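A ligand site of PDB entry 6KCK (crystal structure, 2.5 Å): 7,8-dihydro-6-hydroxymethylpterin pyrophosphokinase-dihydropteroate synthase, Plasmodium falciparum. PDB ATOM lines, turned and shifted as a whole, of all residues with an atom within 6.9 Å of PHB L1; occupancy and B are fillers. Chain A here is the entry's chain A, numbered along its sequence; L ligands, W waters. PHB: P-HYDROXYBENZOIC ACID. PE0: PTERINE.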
ATOM      1  N   SER A 435      15.620 -35.074  16.240  1.00  0.00           N
ATOM      2  CA  SER A 435      14.964 -34.379  17.342  1.00  0.00           C
ATOM      3  C   SER A 435      15.973 -33.768  18.296  1.00  0.00           C
ATOM      4  O   SER A 435      17.021 -34.368  18.589  1.00  0.00           O
ATOM      5  CB  SER A 435      14.033 -35.288  18.116  1.00  0.00           C
ATOM      6  OG  SER A 435      13.412 -34.566  19.178  1.00  0.00           O
ATOM      7  N   SER A 436      15.630 -32.571  18.777  1.00  0.00           N
ATOM      8  CA  SER A 436      16.411 -31.839  19.791  1.00  0.00           C
ATOM      9  C   SER A 436      15.497 -31.579  21.001  1.00  0.00           C
ATOM     10  O   SER A 436      15.855 -30.815  21.907  1.00  0.00           O
ATOM     11  CB  SER A 436      16.949 -30.521  19.224  1.00  0.00           C
ATOM     12  OG  SER A 436      15.890 -29.679  18.707  1.00  0.00           O
ATOM     13  N   ALA A 437      14.329 -32.217  21.003  1.00  0.00           N
ATOM     14  CA  ALA A 437      13.340 -32.083  22.068  1.00  0.00           C
ATOM     15  C   ALA A 437      13.874 -32.544  23.427  1.00  0.00           C
ATOM     16  O   ALA A 437      14.701 -33.443  23.485  1.00  0.00           O
ATOM     17  CB  ALA A 437      12.073 -32.872  21.700  1.00  0.00           C
ATOM     18  N   PRO A 438      13.412 -31.940  24.522  1.00  0.00           N
ATOM     19  CA  PRO A 438      13.930 -32.353  25.845  1.00  0.00           C
ATOM     20  C   PRO A 438      13.999 -33.896  26.075  1.00  0.00           C
ATOM     21  O   PRO A 438      13.005 -34.614  25.924  1.00  0.00           O
ATOM     22  CB  PRO A 438      12.944 -31.696  26.826  1.00  0.00           C
ATOM     23  CG  PRO A 438      11.865 -31.065  25.998  1.00  0.00           C
ATOM     24  CD  PRO A 438      12.428 -30.851  24.629  1.00  0.00           C
ATOM     25  N   ILE A 504      20.707 -25.001  14.905  1.00  0.00           N
ATOM     26  CA  ILE A 504      20.390 -24.746  16.281  1.00  0.00           C
ATOM     27  C   ILE A 504      21.590 -24.527  17.199  1.00  0.00           C
ATOM     28  O   ILE A 504      21.396 -24.173  18.360  1.00  0.00           O
ATOM     29  CB  ILE A 504      19.503 -25.855  16.887  1.00  0.00           C
ATOM     30  CG1 ILE A 504      20.232 -27.221  16.857  1.00  0.00           C
ATOM     31  CG2 ILE A 504      18.156 -25.876  16.161  1.00  0.00           C
ATOM     32  CD1 ILE A 504      19.597 -28.262  17.770  1.00  0.00           C
ATOM     33  N   MET A 538      20.246 -29.266  28.826  1.00  0.00           N
ATOM     34  CA  MET A 538      19.764 -27.903  28.544  1.00  0.00           C
ATOM     35  C   MET A 538      18.784 -27.309  29.556  1.00  0.00           C
ATOM     36  O   MET A 538      18.909 -26.151  29.882  1.00  0.00           O
ATOM     37  CB  MET A 538      19.201 -27.754  27.133  1.00  0.00           C
ATOM     38  CG  MET A 538      17.794 -28.265  26.889  1.00  0.00           C
ATOM     39  SD  MET A 538      17.429 -27.934  25.158  1.00  0.00           S
ATOM     40  CE  MET A 538      15.853 -28.786  24.935  1.00  0.00           C
ATOM     41  N   ASP A 539      17.833 -28.099  30.040  1.00  0.00           N
ATOM     42  CA  ASP A 539      16.918 -27.653  31.100  1.00  0.00           C
ATOM     43  C   ASP A 539      17.653 -27.280  32.396  1.00  0.00           C
ATOM     44  O   ASP A 539      17.109 -26.573  33.230  1.00  0.00           O
ATOM     45  CB  ASP A 539      15.880 -28.721  31.394  1.00  0.00           C
ATOM     46  CG  ASP A 539      14.752 -28.778  30.363  1.00  0.00           C
ATOM     47  OD1 ASP A 539      14.343 -27.725  29.810  1.00  0.00           O
ATOM     48  OD2 ASP A 539      14.237 -29.884  30.148  1.00  0.00           O
ATOM     49  N   LEU A 578      13.492 -20.300  21.768  1.00  0.00           N
ATOM     50  CA  LEU A 578      12.585 -20.476  22.921  1.00  0.00           C
ATOM     51  C   LEU A 578      12.649 -21.920  23.359  1.00  0.00           C
ATOM     52  O   LEU A 578      12.711 -22.825  22.520  1.00  0.00           O
ATOM     53  CB  LEU A 578      11.161 -20.065  22.568  1.00  0.00           C
ATOM     54  CG  LEU A 578      10.976 -18.605  22.138  1.00  0.00           C
ATOM     55  CD1 LEU A 578       9.641 -18.430  21.440  1.00  0.00           C
ATOM     56  CD2 LEU A 578      11.059 -17.641  23.306  1.00  0.00           C
ATOM     57  N   GLY A 579      12.625 -22.177  24.665  1.00  0.00           N
ATOM     58  CA  GLY A 579      12.673 -23.573  25.143  1.00  0.00           C
ATOM     59  C   GLY A 579      14.047 -24.256  25.212  1.00  0.00           C
ATOM     60  O   GLY A 579      14.152 -25.350  25.752  1.00  0.00           O
ATOM     61  N   PHE A 580      15.098 -23.622  24.692  1.00  0.00           N
ATOM     62  CA  PHE A 580      16.433 -24.204  24.720  1.00  0.00           C
ATOM     63  C   PHE A 580      17.321 -23.584  25.779  1.00  0.00           C
ATOM     64  O   PHE A 580      17.966 -22.535  25.515  1.00  0.00           O
ATOM     65  CB  PHE A 580      17.142 -24.031  23.405  1.00  0.00           C
ATOM     66  CG  PHE A 580      16.599 -24.875  22.282  1.00  0.00           C
ATOM     67  CD1 PHE A 580      15.451 -24.470  21.563  1.00  0.00           C
ATOM     68  CD2 PHE A 580      17.278 -26.040  21.891  1.00  0.00           C
ATOM     69  CE1 PHE A 580      14.990 -25.222  20.489  1.00  0.00           C
ATOM     70  CE2 PHE A 580      16.829 -26.783  20.800  1.00  0.00           C
ATOM     71  CZ  PHE A 580      15.692 -26.362  20.086  1.00  0.00           C
ATOM     72  N   LYS A 582      16.095 -22.453  28.610  1.00  0.00           N
ATOM     73  CA  LYS A 582      15.270 -21.389  29.121  1.00  0.00           C
ATOM     74  C   LYS A 582      14.179 -22.009  29.948  1.00  0.00           C
ATOM     75  O   LYS A 582      13.518 -22.916  29.496  1.00  0.00           O
ATOM     76  CB  LYS A 582      14.642 -20.614  27.950  1.00  0.00           C
ATOM     77  CG  LYS A 582      15.333 -19.321  27.569  1.00  0.00           C
ATOM     78  CD  LYS A 582      16.606 -19.504  26.760  1.00  0.00           C
ATOM     79  CE  LYS A 582      16.389 -19.622  25.262  1.00  0.00           C
ATOM     80  NZ  LYS A 582      17.650 -19.741  24.475  1.00  0.00           N
ATOM     81  N   HIS A 584      10.373 -21.674  31.538  1.00  0.00           N
ATOM     82  CA  HIS A 584       9.214 -21.107  30.878  1.00  0.00           C
ATOM     83  C   HIS A 584       9.068 -19.633  31.023  1.00  0.00           C
ATOM     84  O   HIS A 584       8.753 -18.952  30.032  1.00  0.00           O
ATOM     85  CB  HIS A 584       7.996 -21.860  31.305  1.00  0.00           C
ATOM     86  CG  HIS A 584       8.120 -23.351  31.065  1.00  0.00           C
ATOM     87  ND1 HIS A 584       8.939 -23.877  30.103  1.00  0.00           N
ATOM     88  CD2 HIS A 584       7.502 -24.439  31.702  1.00  0.00           C
ATOM     89  CE1 HIS A 584       8.859 -25.222  30.147  1.00  0.00           C
ATOM     90  NE2 HIS A 584       7.963 -25.567  31.111  1.00  0.00           N
ATOM     91  N   SER A 587      11.514 -18.064  28.610  1.00  0.00           N
ATOM     92  CA  SER A 587      10.949 -18.045  27.254  1.00  0.00           C
ATOM     93  C   SER A 587       9.958 -16.871  27.032  1.00  0.00           C
ATOM     94  O   SER A 587      10.079 -16.127  26.062  1.00  0.00           O
ATOM     95  CB  SER A 587      10.310 -19.364  26.913  1.00  0.00           C
ATOM     96  OG  SER A 587      11.338 -20.287  26.629  1.00  0.00           O
ATOM     97  N   TYR A 606       8.035 -21.195  18.474  1.00  0.00           N
ATOM     98  CA  TYR A 606       7.383 -21.359  19.758  1.00  0.00           C
ATOM     99  C   TYR A 606       6.516 -22.600  19.688  1.00  0.00           C
ATOM    100  O   TYR A 606       6.074 -23.094  20.710  1.00  0.00           O
ATOM    101  CB  TYR A 606       6.519 -20.129  20.028  1.00  0.00           C
ATOM    102  CG  TYR A 606       5.546 -19.846  18.897  1.00  0.00           C
ATOM    103  CD1 TYR A 606       4.332 -20.555  18.791  1.00  0.00           C
ATOM    104  CD2 TYR A 606       5.807 -18.865  17.943  1.00  0.00           C
ATOM    105  CE1 TYR A 606       3.441 -20.302  17.775  1.00  0.00           C
ATOM    106  CE2 TYR A 606       4.910 -18.591  16.916  1.00  0.00           C
ATOM    107  CZ  TYR A 606       3.732 -19.323  16.844  1.00  0.00           C
ATOM    108  OH  TYR A 606       2.838 -19.092  15.825  1.00  0.00           O
ATOM    109  N   SER A 607       6.301 -23.112  18.477  1.00  0.00           N
ATOM    110  CA  SER A 607       5.208 -24.081  18.229  1.00  0.00           C
ATOM    111  C   SER A 607       5.249 -25.364  19.066  1.00  0.00           C
ATOM    112  O   SER A 607       6.239 -26.144  19.034  1.00  0.00           O
ATOM    113  CB  SER A 607       5.102 -24.417  16.749  1.00  0.00           C
ATOM    114  OG  SER A 607       4.145 -25.451  16.572  1.00  0.00           O
ATOM    115  N   ARG A 608       4.160 -25.597  19.811  1.00  0.00           N
ATOM    116  CA  ARG A 608       3.991 -26.793  20.658  1.00  0.00           C
ATOM    117  C   ARG A 608       5.083 -26.978  21.702  1.00  0.00           C
ATOM    118  O   ARG A 608       5.320 -28.094  22.153  1.00  0.00           O
ATOM    119  CB  ARG A 608       3.882 -28.069  19.816  1.00  0.00           C
ATOM    120  CG  ARG A 608       2.590 -28.080  19.026  1.00  0.00           C
ATOM    121  CD  ARG A 608       2.539 -29.254  18.094  1.00  0.00           C
ATOM    122  NE  ARG A 608       1.443 -29.120  17.141  1.00  0.00           N
ATOM    123  CZ  ARG A 608       1.070 -30.102  16.323  1.00  0.00           C
ATOM    124  NH1 ARG A 608       1.694 -31.277  16.382  1.00  0.00           N
ATOM    125  NH2 ARG A 608       0.083 -29.936  15.468  1.00  0.00           N
ATOM    126  N   LYS A 609       5.741 -25.892  22.069  1.00  0.00           N
ATOM    127  CA  LYS A 609       6.747 -25.977  23.096  1.00  0.00           C
ATOM    128  C   LYS A 609       6.078 -25.907  24.464  1.00  0.00           C
ATOM    129  O   LYS A 609       4.971 -25.397  24.606  1.00  0.00           O
ATOM    130  CB  LYS A 609       7.813 -24.876  22.913  1.00  0.00           C
ATOM    131  CG  LYS A 609       8.623 -25.038  21.615  1.00  0.00           C
ATOM    132  CD  LYS A 609      10.019 -24.464  21.762  1.00  0.00           C
ATOM    133  CE  LYS A 609      10.958 -25.050  20.734  1.00  0.00           C
ATOM    134  NZ  LYS A 609      11.381 -24.071  19.682  1.00  0.00           N
ATOM    135  N   ARG A 610       6.759 -26.452  25.466  1.00  0.00           N
ATOM    136  CA  ARG A 610       6.272 -26.525  26.820  1.00  0.00           C
ATOM    137  C   ARG A 610       5.836 -25.213  27.411  1.00  0.00           C
ATOM    138  O   ARG A 610       4.834 -25.181  28.121  1.00  0.00           O
ATOM    139  CB  ARG A 610       7.359 -27.133  27.717  1.00  0.00           C
ATOM    140  CG  ARG A 610       7.602 -28.619  27.448  1.00  0.00           C
ATOM    141  CD  ARG A 610       8.885 -29.110  28.074  1.00  0.00           C
ATOM    142  NE  ARG A 610      10.039 -28.345  27.591  1.00  0.00           N
ATOM    143  CZ  ARG A 610      11.227 -28.299  28.183  1.00  0.00           C
ATOM    144  NH1 ARG A 610      11.453 -28.995  29.289  1.00  0.00           N
ATOM    145  NH2 ARG A 610      12.205 -27.562  27.651  1.00  0.00           N
ATOM    146  N   PHE A 611       6.564 -24.130  27.138  1.00  0.00           N
ATOM    147  CA  PHE A 611       6.270 -22.860  27.836  1.00  0.00           C
ATOM    148  C   PHE A 611       4.851 -22.328  27.557  1.00  0.00           C
ATOM    149  O   PHE A 611       4.322 -21.511  28.328  1.00  0.00           O
ATOM    150  CB  PHE A 611       7.329 -21.789  27.529  1.00  0.00           C
ATOM    151  CG  PHE A 611       7.155 -21.091  26.196  1.00  0.00           C
ATOM    152  CD1 PHE A 611       7.711 -21.637  25.033  1.00  0.00           C
ATOM    153  CD2 PHE A 611       6.462 -19.884  26.101  1.00  0.00           C
ATOM    154  CE1 PHE A 611       7.538 -21.011  23.803  1.00  0.00           C
ATOM    155  CE2 PHE A 611       6.328 -19.244  24.865  1.00  0.00           C
ATOM    156  CZ  PHE A 611       6.865 -19.808  23.716  1.00  0.00           C
ATOM    157  N   ARG A 686       8.221 -20.404  12.861  1.00  0.00           N
ATOM    158  CA  ARG A 686       8.349 -21.829  12.606  1.00  0.00           C
ATOM    159  C   ARG A 686       7.232 -22.625  13.337  1.00  0.00           C
ATOM    160  O   ARG A 686       7.208 -22.695  14.569  1.00  0.00           O
ATOM    161  CB  ARG A 686       9.717 -22.270  13.096  1.00  0.00           C
ATOM    162  CG  ARG A 686      10.014 -23.741  12.859  1.00  0.00           C
ATOM    163  CD  ARG A 686      11.407 -24.071  13.377  1.00  0.00           C
ATOM    164  NE  ARG A 686      11.729 -25.465  13.123  1.00  0.00           N
ATOM    165  CZ  ARG A 686      11.395 -26.465  13.940  1.00  0.00           C
ATOM    166  NH1 ARG A 686      10.725 -26.237  15.092  1.00  0.00           N
ATOM    167  NH2 ARG A 686      11.725 -27.693  13.581  1.00  0.00           N
HETATM  168  C1' PHB L   1      10.245 -27.461  24.430  1.00  0.00           C
HETATM  169  O1' PHB L   1       9.041 -27.869  24.411  1.00  0.00           O
HETATM  170  O2' PHB L   1      10.719 -26.757  25.356  1.00  0.00           O
HETATM  171  C1  PHB L   1      11.152 -27.873  23.315  1.00  0.00           C
HETATM  172  C2  PHB L   1      12.472 -27.483  23.303  1.00  0.00           C
HETATM  173  C3  PHB L   1      13.306 -27.893  22.256  1.00  0.00           C
HETATM  174  C4  PHB L   1      12.783 -28.698  21.241  1.00  0.00           C
HETATM  175  C5  PHB L   1      11.438 -29.099  21.265  1.00  0.00           C
HETATM  176  C6  PHB L   1      10.643 -28.676  22.305  1.00  0.00           C
HETATM  177  O4  PHB L   1      13.584 -29.112  20.203  1.00  0.00           O
HETATM  178  C1  PE0 L   2      13.427 -24.764  16.917  1.00  0.00           C
HETATM  179  C4  PE0 L   2      13.444 -23.322  17.090  1.00  0.00           C
HETATM  180  O4  PE0 L   2      12.756 -22.803  17.996  1.00  0.00           O
HETATM  181  N2  PE0 L   2      14.201 -22.598  16.248  1.00  0.00           N
HETATM  182  C3  PE0 L   2      14.949 -23.157  15.266  1.00  0.00           C
HETATM  183  N6  PE0 L   2      15.696 -22.306  14.514  1.00  0.00           N
HETATM  184  N1  PE0 L   2      14.962 -24.501  15.035  1.00  0.00           N
HETATM  185  C2  PE0 L   2      14.244 -25.333  15.822  1.00  0.00           C
HETATM  186  N3  PE0 L   2      14.230 -26.695  15.666  1.00  0.00           N
HETATM  187  C6  PE0 L   2      13.459 -27.450  16.480  1.00  0.00           C
HETATM  188  C5  PE0 L   2      12.699 -26.893  17.531  1.00  0.00           C
HETATM  189  N4  PE0 L   2      12.674 -25.551  17.715  1.00  0.00           N
HETATM  190  O   HOH W   1       8.019 -30.323  23.978  1.00  0.00           O
HETATM  191  O   HOH W   2       9.382 -24.530  26.302  1.00  0.00           O
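Water W2 lies within hydrogen-bond range of an oxygen (O2') of PHB L1 (2.8 Å), the backbone NH of Phe 611 (3.0 Å) and the backbone NH of Arg 610 (3.4 Å).
N of Ala 437 is in hydrogen-bond range of O4 of PHB L1 (3.3 Å).
O2' of PHB L1 is in salt-bridge range of NE of Arg 610, 2.8 Å away.
The backbone NH (N) of Arg 610 lies within hydrogen-bond range of an oxygen (O1') of PHB L1, at 2.9 Å.
N4 of PE0 L2 sits close to NH1 of Arg 686 (3.3 Å).
The backbone carbonyl oxygen (O) of Ser 436 sits close to an oxygen (O4) of PHB L1 (3.3 Å).
An oxygen (O4) of PHB L1 is in hydrogen-bond range of the side-chain hydroxyl of Ser 436 (2.8 Å).
An oxygen (O4) of PE0 L2 is in hydrogen-bond range of the side-chain amino group (NZ) of Lys 609 (2.5 Å).
Merely in contact with PHB L1: Pro 438 (3.5 Å), Met 538 (3.8 Å), Gly 579 (3.7 Å), Phe 580 (3.5 Å) and Lys 609 (3.3 Å).
Hydrophobic or aromatic side chains that line PHB L1: Ala 437, Pro 438, Met 538 and Phe 580.
Of the 20 residues printed, 8 come within 4 Å of PHB L1.
The nearest printed residue that does not touch PHB L1 is Arg 608 (4.4 Å).
N of Ala 437 lies within hydrogen-bond range of OG of Ser 435, 3.1 Å away.
NH2 of Arg 610 lies within salt-bridge range of OD1 of Asp 539 (3.0 Å).
The backbone carbonyl oxygen of Phe 580 sits at hydrogen-bond distance from the side-chain amino group of Lys 582 (3.0 Å).
The backbone NH of Gly 579 sits at hydrogen-bond distance from the side-chain hydroxyl of Ser 587 (3.0 Å).
The side-chain amino group (NZ) of Lys 609 sits close to the backbone carbonyl oxygen (O) of Leu 578, 3.4 Å away.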
